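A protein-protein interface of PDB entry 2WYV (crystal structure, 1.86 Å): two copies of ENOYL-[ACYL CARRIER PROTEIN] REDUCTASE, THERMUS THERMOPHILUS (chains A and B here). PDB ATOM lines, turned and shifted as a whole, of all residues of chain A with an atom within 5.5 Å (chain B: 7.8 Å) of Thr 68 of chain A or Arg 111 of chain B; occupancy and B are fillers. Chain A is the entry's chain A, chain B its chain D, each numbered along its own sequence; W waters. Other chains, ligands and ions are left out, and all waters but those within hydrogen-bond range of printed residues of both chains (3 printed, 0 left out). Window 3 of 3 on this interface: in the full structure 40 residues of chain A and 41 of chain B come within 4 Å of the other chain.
The backbone carbonyl oxygen (O) of Val 67 of chain A lies within hydrogen-bond range of the guanidinium group (NH2) of Arg 111 of chain B.
The side-chain carboxylate (OD2) of Asp 70 of chain A lies within salt-bridge range of the guanidinium group (NH2) of Arg 111 of chain B.
The side-chain carboxylate of Glu 119 of chain A lies within salt-bridge range of the guanidinium group of Arg 111 of chain B (2.9 Å).
O of Thr 109 of chain B sits at hydrogen-bond distance from OH of Tyr 123 of chain A, at 2.8 Å.
OH of Tyr 123 of chain A sits at hydrogen-bond distance from N of Arg 111 of chain B.
The side-chain carboxylate of Asp 66 of chain A sits at hydrogen-bond distance from the side-chain hydroxyl of Thr 68 of chain A, 2.8 Å away.
The side-chain hydroxyl (OG1) of Thr 68 of chain A sits at hydrogen-bond distance from the side-chain amide oxygen (OE1) of Gln 69 of chain A, 3.3 Å away.
The side-chain carboxylate of Asp 113 of chain B lies within salt-bridge range of the guanidinium group of Arg 110 of chain B (3.1 Å).
Thr 68 of chain A touches Arg 111 of chain B (O to CZ, 3.5 Å).
CB of Glu 119 of chain A touches CD2 of Leu 115 of chain B (3.9 Å).
Arg 110 of chain B touches Tyr 123 of chain A (C to OH, 3.6 Å).
Tyr 123 of chain A touches Trp 114 of chain B (CD1 to CG, 3.4 Å).
Printed residues of chain B within 4 Å of Val 67 of chain A: Arg 111 (2.9 Å).
Of chain B, only Arg 111 (3.5 Å) comes within 4 Å of Thr 68 of chain A.
Gln 69 of chain A touches none of the printed residues of chain B.
Printed residues of chain A within 4 Å of Arg 110 of chain B: Tyr 123.
Of chain A, only Val 67, Thr 68, Asp 70, Glu 119 and Tyr 123 come within 4 Å of Arg 111 of chain B.
Of the printed residues of chain A, Trp 114 of chain B touches Tyr 123 (3.4 Å).
The nearest residue of chain B that does not touch Thr 68 of chain A is Gln 112 of chain B (6.9 Å).
The nearest printed residue of chain A that does not touch Arg 111 of chain B is Leu 73 of chain A (4.2 Å).
Hydrophobic or aromatic side chains of chain A within 4 Å of the printed part of chain B: Tyr 123.
Along chain A the printed residues that touch a printed residue of chain B span positions 67 to 123.
Of the 10 printed residues of chain B, 5 touch a printed residue of chain A.
Among the printed residues, 9 pairs touch across the chains.
1 position is printed for both chains.
Water W2 lies within hydrogen-bond range of NE2 of Gln 112 of chain B (2.6 Å) and OE1 of Glu 119 of chain A (3.3 Å).
Water W1 lies within hydrogen-bond range of O of Glu 119 of chain A (2.7 Å), NH1 of Arg 111 of chain B (2.9 Å) and O of Val 67 of chain A (3.0 Å).
Water W3 lies within hydrogen-bond range of the side-chain carboxylate of Asp 70 of chain A (3.0 Å) and the backbone NH of Arg 111 of chain B (3.1 Å).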
ATOM      1  N   ASP A  66      -4.771 -21.771 -38.696  1.00  0.00           N
ATOM      2  CA  ASP A  66      -5.340 -20.486 -38.293  1.00  0.00           C
ATOM      3  C   ASP A  66      -5.546 -20.548 -36.777  1.00  0.00           C
ATOM      4  O   ASP A  66      -6.228 -21.451 -36.294  1.00  0.00           O
ATOM      5  CB  ASP A  66      -6.670 -20.266 -39.008  1.00  0.00           C
ATOM      6  CG  ASP A  66      -7.321 -18.889 -38.696  1.00  0.00           C
ATOM      7  OD1 ASP A  66      -7.766 -18.248 -39.660  1.00  0.00           O
ATOM      8  OD2 ASP A  66      -7.431 -18.446 -37.535  1.00  0.00           O
ATOM      9  N   VAL A  67      -4.964 -19.592 -36.039  1.00  0.00           N
ATOM     10  CA  VAL A  67      -4.940 -19.638 -34.559  1.00  0.00           C
ATOM     11  C   VAL A  67      -6.308 -19.384 -33.919  1.00  0.00           C
ATOM     12  O   VAL A  67      -6.452 -19.575 -32.727  1.00  0.00           O
ATOM     13  CB  VAL A  67      -3.952 -18.651 -33.925  1.00  0.00           C
ATOM     14  CG1 VAL A  67      -2.551 -19.030 -34.281  1.00  0.00           C
ATOM     15  CG2 VAL A  67      -4.285 -17.144 -34.336  1.00  0.00           C
ATOM     16  N   THR A  68      -7.317 -19.011 -34.698  1.00  0.00           N
ATOM     17  CA  THR A  68      -8.657 -18.960 -34.160  1.00  0.00           C
ATOM     18  C   THR A  68      -9.344 -20.335 -34.216  1.00  0.00           C
ATOM     19  O   THR A  68     -10.439 -20.457 -33.696  1.00  0.00           O
ATOM     20  CB  THR A  68      -9.526 -17.859 -34.807  1.00  0.00           C
ATOM     21  OG1 THR A  68      -9.871 -18.239 -36.141  1.00  0.00           O
ATOM     22  CG2 THR A  68      -8.789 -16.538 -34.781  1.00  0.00           C
ATOM     23  N   GLN A  69      -8.685 -21.369 -34.766  1.00  0.00           N
ATOM     24  CA  GLN A  69      -9.318 -22.701 -34.925  1.00  0.00           C
ATOM     25  C   GLN A  69      -8.621 -23.797 -34.129  1.00  0.00           C
ATOM     26  O   GLN A  69      -7.538 -24.247 -34.504  1.00  0.00           O
ATOM     27  CB  GLN A  69      -9.357 -23.067 -36.414  1.00  0.00           C
ATOM     28  CG  GLN A  69     -10.030 -22.017 -37.282  1.00  0.00           C
ATOM     29  CD  GLN A  69     -11.508 -21.792 -36.928  1.00  0.00           C
ATOM     30  OE1 GLN A  69     -11.969 -20.659 -36.813  1.00  0.00           O
ATOM     31  NE2 GLN A  69     -12.231 -22.871 -36.710  1.00  0.00           N
ATOM     32  N   ASP A  70      -9.242 -24.240 -33.026  1.00  0.00           N
ATOM     33  CA  ASP A  70      -8.593 -25.163 -32.093  1.00  0.00           C
ATOM     34  C   ASP A  70      -8.171 -26.538 -32.665  1.00  0.00           C
ATOM     35  O   ASP A  70      -7.114 -27.072 -32.293  1.00  0.00           O
ATOM     36  CB  ASP A  70      -9.483 -25.368 -30.852  1.00  0.00           C
ATOM     37  CG  ASP A  70      -9.448 -24.171 -29.896  1.00  0.00           C
ATOM     38  OD1 ASP A  70     -10.508 -23.810 -29.388  1.00  0.00           O
ATOM     39  OD2 ASP A  70      -8.371 -23.594 -29.642  1.00  0.00           O
ATOM     40  N   LEU A  73      -5.067 -26.135 -34.612  1.00  0.00           N
ATOM     41  CA  LEU A  73      -3.919 -26.015 -33.714  1.00  0.00           C
ATOM     42  C   LEU A  73      -3.510 -27.388 -33.227  1.00  0.00           C
ATOM     43  O   LEU A  73      -2.318 -27.683 -33.122  1.00  0.00           O
ATOM     44  CB  LEU A  73      -4.248 -25.115 -32.517  1.00  0.00           C
ATOM     45  CG  LEU A  73      -4.072 -23.610 -32.761  1.00  0.00           C
ATOM     46  CD1 LEU A  73      -4.771 -23.216 -34.016  1.00  0.00           C
ATOM     47  CD2 LEU A  73      -4.607 -22.799 -31.601  1.00  0.00           C
ATOM     48  N   LEU A 116     -12.471  -9.920 -31.739  1.00  0.00           N
ATOM     49  CA  LEU A 116     -11.537 -10.553 -32.690  1.00  0.00           C
ATOM     50  C   LEU A 116     -10.074 -10.080 -32.511  1.00  0.00           C
ATOM     51  O   LEU A 116      -9.167 -10.898 -32.588  1.00  0.00           O
ATOM     52  CB  LEU A 116     -11.966 -10.391 -34.155  1.00  0.00           C
ATOM     53  CG  LEU A 116     -11.220 -11.200 -35.248  1.00  0.00           C
ATOM     54  CD1 LEU A 116     -11.172 -12.689 -35.037  1.00  0.00           C
ATOM     55  CD2 LEU A 116     -11.846 -10.869 -36.609  1.00  0.00           C
ATOM     56  N   GLU A 119      -8.904 -11.881 -29.393  1.00  0.00           N
ATOM     57  CA  GLU A 119      -8.772 -13.364 -29.665  1.00  0.00           C
ATOM     58  C   GLU A 119      -7.481 -13.690 -30.436  1.00  0.00           C
ATOM     59  O   GLU A 119      -6.707 -14.594 -30.102  1.00  0.00           O
ATOM     60  CB  GLU A 119      -9.995 -13.854 -30.469  1.00  0.00           C
ATOM     61  CG  GLU A 119     -10.115 -15.405 -30.582  1.00  0.00           C
ATOM     62  CD  GLU A 119     -11.288 -15.857 -31.458  1.00  0.00           C
ATOM     63  OE1 GLU A 119     -11.497 -17.085 -31.557  1.00  0.00           O
ATOM     64  OE2 GLU A 119     -11.977 -15.002 -32.055  1.00  0.00           O
ATOM     65  N   VAL A 120      -7.226 -12.911 -31.485  1.00  0.00           N
ATOM     66  CA  VAL A 120      -6.066 -13.138 -32.335  1.00  0.00           C
ATOM     67  C   VAL A 120      -4.738 -12.621 -31.691  1.00  0.00           C
ATOM     68  O   VAL A 120      -3.727 -13.286 -31.770  1.00  0.00           O
ATOM     69  CB  VAL A 120      -6.255 -12.495 -33.768  1.00  0.00           C
ATOM     70  CG1 VAL A 120      -5.022 -12.723 -34.662  1.00  0.00           C
ATOM     71  CG2 VAL A 120      -7.518 -13.084 -34.533  1.00  0.00           C
ATOM     72  N   TYR A 123      -5.284 -13.998 -26.887  1.00  0.00           N
ATOM     73  CA  TYR A 123      -5.662 -15.401 -26.546  1.00  0.00           C
ATOM     74  C   TYR A 123      -4.799 -16.448 -27.265  1.00  0.00           C
ATOM     75  O   TYR A 123      -4.525 -17.537 -26.723  1.00  0.00           O
ATOM     76  CB  TYR A 123      -7.165 -15.690 -26.756  1.00  0.00           C
ATOM     77  CG  TYR A 123      -7.496 -17.139 -26.357  1.00  0.00           C
ATOM     78  CD1 TYR A 123      -7.451 -17.540 -25.026  1.00  0.00           C
ATOM     79  CD2 TYR A 123      -7.739 -18.104 -27.313  1.00  0.00           C
ATOM     80  CE1 TYR A 123      -7.677 -18.888 -24.646  1.00  0.00           C
ATOM     81  CE2 TYR A 123      -7.981 -19.473 -26.946  1.00  0.00           C
ATOM     82  CZ  TYR A 123      -7.953 -19.837 -25.604  1.00  0.00           C
ATOM     83  OH  TYR A 123      -8.180 -21.162 -25.242  1.00  0.00           O
ATOM     84  N   ALA A 127      -3.452 -20.361 -26.260  1.00  0.00           N
ATOM     85  CA  ALA A 127      -3.800 -21.520 -27.118  1.00  0.00           C
ATOM     86  C   ALA A 127      -2.557 -22.302 -27.573  1.00  0.00           C
ATOM     87  O   ALA A 127      -2.546 -23.523 -27.550  1.00  0.00           O
ATOM     88  CB  ALA A 127      -4.601 -21.066 -28.331  1.00  0.00           C
ATOM     89  N   ASP B 108      -4.672 -23.504 -19.096  1.00  0.00           N
ATOM     90  CA  ASP B 108      -5.744 -24.436 -19.444  1.00  0.00           C
ATOM     91  C   ASP B 108      -7.097 -23.771 -19.765  1.00  0.00           C
ATOM     92  O   ASP B 108      -8.086 -24.473 -19.982  1.00  0.00           O
ATOM     93  CB  ASP B 108      -5.937 -25.449 -18.288  1.00  0.00           C
ATOM     94  CG  ASP B 108      -4.771 -26.409 -18.137  1.00  0.00           C
ATOM     95  OD1 ASP B 108      -4.545 -26.910 -17.006  1.00  0.00           O
ATOM     96  OD2 ASP B 108      -4.079 -26.694 -19.129  1.00  0.00           O
ATOM     97  N   THR B 109      -7.176 -22.432 -19.809  1.00  0.00           N
ATOM     98  CA  THR B 109      -8.455 -21.757 -20.121  1.00  0.00           C
ATOM     99  C   THR B 109      -9.014 -22.023 -21.526  1.00  0.00           C
ATOM    100  O   THR B 109      -8.349 -21.783 -22.544  1.00  0.00           O
ATOM    101  CB  THR B 109      -8.338 -20.174 -20.005  1.00  0.00           C
ATOM    102  OG1 THR B 109      -7.574 -19.836 -18.851  1.00  0.00           O
ATOM    103  CG2 THR B 109      -9.714 -19.515 -19.972  1.00  0.00           C
ATOM    104  N   ARG B 110     -10.277 -22.444 -21.568  1.00  0.00           N
ATOM    105  CA  ARG B 110     -11.010 -22.644 -22.820  1.00  0.00           C
ATOM    106  C   ARG B 110     -11.326 -21.327 -23.518  1.00  0.00           C
ATOM    107  O   ARG B 110     -11.686 -20.339 -22.864  1.00  0.00           O
ATOM    108  CB  ARG B 110     -12.314 -23.412 -22.539  1.00  0.00           C
ATOM    109  CG  ARG B 110     -12.078 -24.833 -22.011  1.00  0.00           C
ATOM    110  CD  ARG B 110     -13.399 -25.567 -21.779  1.00  0.00           C
ATOM    111  NE  ARG B 110     -14.169 -25.038 -20.649  1.00  0.00           N
ATOM    112  CZ  ARG B 110     -15.369 -25.491 -20.256  1.00  0.00           C
ATOM    113  NH1 ARG B 110     -15.969 -26.504 -20.897  1.00  0.00           N
ATOM    114  NH2 ARG B 110     -15.983 -24.933 -19.213  1.00  0.00           N
ATOM    115  N   ARG B 111     -11.220 -21.336 -24.852  1.00  0.00           N
ATOM    116  CA  ARG B 111     -11.445 -20.141 -25.710  1.00  0.00           C
ATOM    117  C   ARG B 111     -12.713 -19.337 -25.421  1.00  0.00           C
ATOM    118  O   ARG B 111     -12.680 -18.094 -25.291  1.00  0.00           O
ATOM    119  CB  ARG B 111     -11.461 -20.590 -27.175  1.00  0.00           C
ATOM    120  CG  ARG B 111     -11.624 -19.511 -28.212  1.00  0.00           C
ATOM    121  CD  ARG B 111     -11.625 -20.116 -29.609  1.00  0.00           C
ATOM    122  NE  ARG B 111     -10.340 -20.734 -29.939  1.00  0.00           N
ATOM    123  CZ  ARG B 111      -9.267 -20.091 -30.406  1.00  0.00           C
ATOM    124  NH1 ARG B 111      -9.293 -18.785 -30.638  1.00  0.00           N
ATOM    125  NH2 ARG B 111      -8.144 -20.774 -30.634  1.00  0.00           N
ATOM    126  N   GLN B 112     -13.853 -20.021 -25.392  1.00  0.00           N
ATOM    127  CA  GLN B 112     -15.115 -19.308 -25.153  1.00  0.00           C
ATOM    128  C   GLN B 112     -15.229 -18.738 -23.727  1.00  0.00           C
ATOM    129  O   GLN B 112     -15.763 -17.661 -23.545  1.00  0.00           O
ATOM    130  CB  GLN B 112     -16.335 -20.172 -25.558  1.00  0.00           C
ATOM    131  CG  GLN B 112     -16.487 -20.369 -27.121  1.00  0.00           C
ATOM    132  CD  GLN B 112     -16.241 -19.096 -28.026  1.00  0.00           C
ATOM    133  OE1 GLN B 112     -16.921 -18.045 -27.897  1.00  0.00           O
ATOM    134  NE2 GLN B 112     -15.290 -19.226 -28.971  1.00  0.00           N
ATOM    135  N   ASP B 113     -14.716 -19.446 -22.719  1.00  0.00           N
ATOM    136  CA  ASP B 113     -14.629 -18.898 -21.362  1.00  0.00           C
ATOM    137  C   ASP B 113     -13.768 -17.605 -21.298  1.00  0.00           C
ATOM    138  O   ASP B 113     -14.171 -16.617 -20.663  1.00  0.00           O
ATOM    139  CB  ASP B 113     -14.102 -19.944 -20.383  1.00  0.00           C
ATOM    140  CG  ASP B 113     -15.062 -21.117 -20.187  1.00  0.00           C
ATOM    141  OD1 ASP B 113     -14.648 -22.155 -19.607  1.00  0.00           O
ATOM    142  OD2 ASP B 113     -16.231 -20.999 -20.601  1.00  0.00           O
ATOM    143  N   TRP B 114     -12.609 -17.626 -21.974  1.00  0.00           N
ATOM    144  CA  TRP B 114     -11.657 -16.483 -21.967  1.00  0.00           C
ATOM    145  C   TRP B 114     -12.281 -15.288 -22.653  1.00  0.00           C
ATOM    146  O   TRP B 114     -12.241 -14.153 -22.142  1.00  0.00           O
ATOM    147  CB  TRP B 114     -10.363 -16.895 -22.670  1.00  0.00           C
ATOM    148  CG  TRP B 114      -9.191 -15.974 -22.614  1.00  0.00           C
ATOM    149  CD1 TRP B 114      -8.090 -16.084 -21.829  1.00  0.00           C
ATOM    150  CD2 TRP B 114      -8.951 -14.832 -23.472  1.00  0.00           C
ATOM    151  NE1 TRP B 114      -7.183 -15.069 -22.118  1.00  0.00           N
ATOM    152  CE2 TRP B 114      -7.697 -14.291 -23.114  1.00  0.00           C
ATOM    153  CE3 TRP B 114      -9.685 -14.222 -24.483  1.00  0.00           C
ATOM    154  CZ2 TRP B 114      -7.158 -13.159 -23.738  1.00  0.00           C
ATOM    155  CZ3 TRP B 114      -9.164 -13.095 -25.101  1.00  0.00           C
ATOM    156  CH2 TRP B 114      -7.904 -12.581 -24.725  1.00  0.00           C
ATOM    157  N   LEU B 115     -12.894 -15.539 -23.810  1.00  0.00           N
ATOM    158  CA  LEU B 115     -13.617 -14.485 -24.526  1.00  0.00           C
ATOM    159  C   LEU B 115     -14.767 -13.912 -23.680  1.00  0.00           C
ATOM    160  O   LEU B 115     -14.915 -12.686 -23.561  1.00  0.00           O
ATOM    161  CB  LEU B 115     -14.079 -14.969 -25.897  1.00  0.00           C
ATOM    162  CG  LEU B 115     -12.934 -15.169 -26.909  1.00  0.00           C
ATOM    163  CD1 LEU B 115     -13.412 -15.991 -28.054  1.00  0.00           C
ATOM    164  CD2 LEU B 115     -12.366 -13.782 -27.407  1.00  0.00           C
ATOM    165  N   LEU B 116     -15.547 -14.767 -23.020  1.00  0.00           N
ATOM    166  CA  LEU B 116     -16.644 -14.236 -22.207  1.00  0.00           C
ATOM    167  C   LEU B 116     -16.131 -13.355 -21.059  1.00  0.00           C
ATOM    168  O   LEU B 116     -16.705 -12.277 -20.772  1.00  0.00           O
ATOM    169  CB  LEU B 116     -17.494 -15.369 -21.631  1.00  0.00           C
ATOM    170  CG  LEU B 116     -18.780 -14.947 -20.924  1.00  0.00           C
ATOM    171  CD1 LEU B 116     -19.663 -14.026 -21.751  1.00  0.00           C
ATOM    172  CD2 LEU B 116     -19.530 -16.257 -20.539  1.00  0.00           C
ATOM    173  N   ALA B 117     -15.063 -13.821 -20.406  1.00  0.00           N
ATOM    174  CA  ALA B 117     -14.459 -13.083 -19.293  1.00  0.00           C
ATOM    175  C   ALA B 117     -14.034 -11.682 -19.745  1.00  0.00           C
ATOM    176  O   ALA B 117     -14.332 -10.706 -19.088  1.00  0.00           O
ATOM    177  CB  ALA B 117     -13.277 -13.835 -18.714  1.00  0.00           C
HETATM  178  O   HOH W   1      -6.874 -17.158 -30.967  1.00  0.00           O
HETATM  179  O   HOH W   2     -14.669 -17.736 -30.979  1.00  0.00           O
HETATM  180  O   HOH W   3     -10.607 -23.931 -26.347  1.00  0.00           O
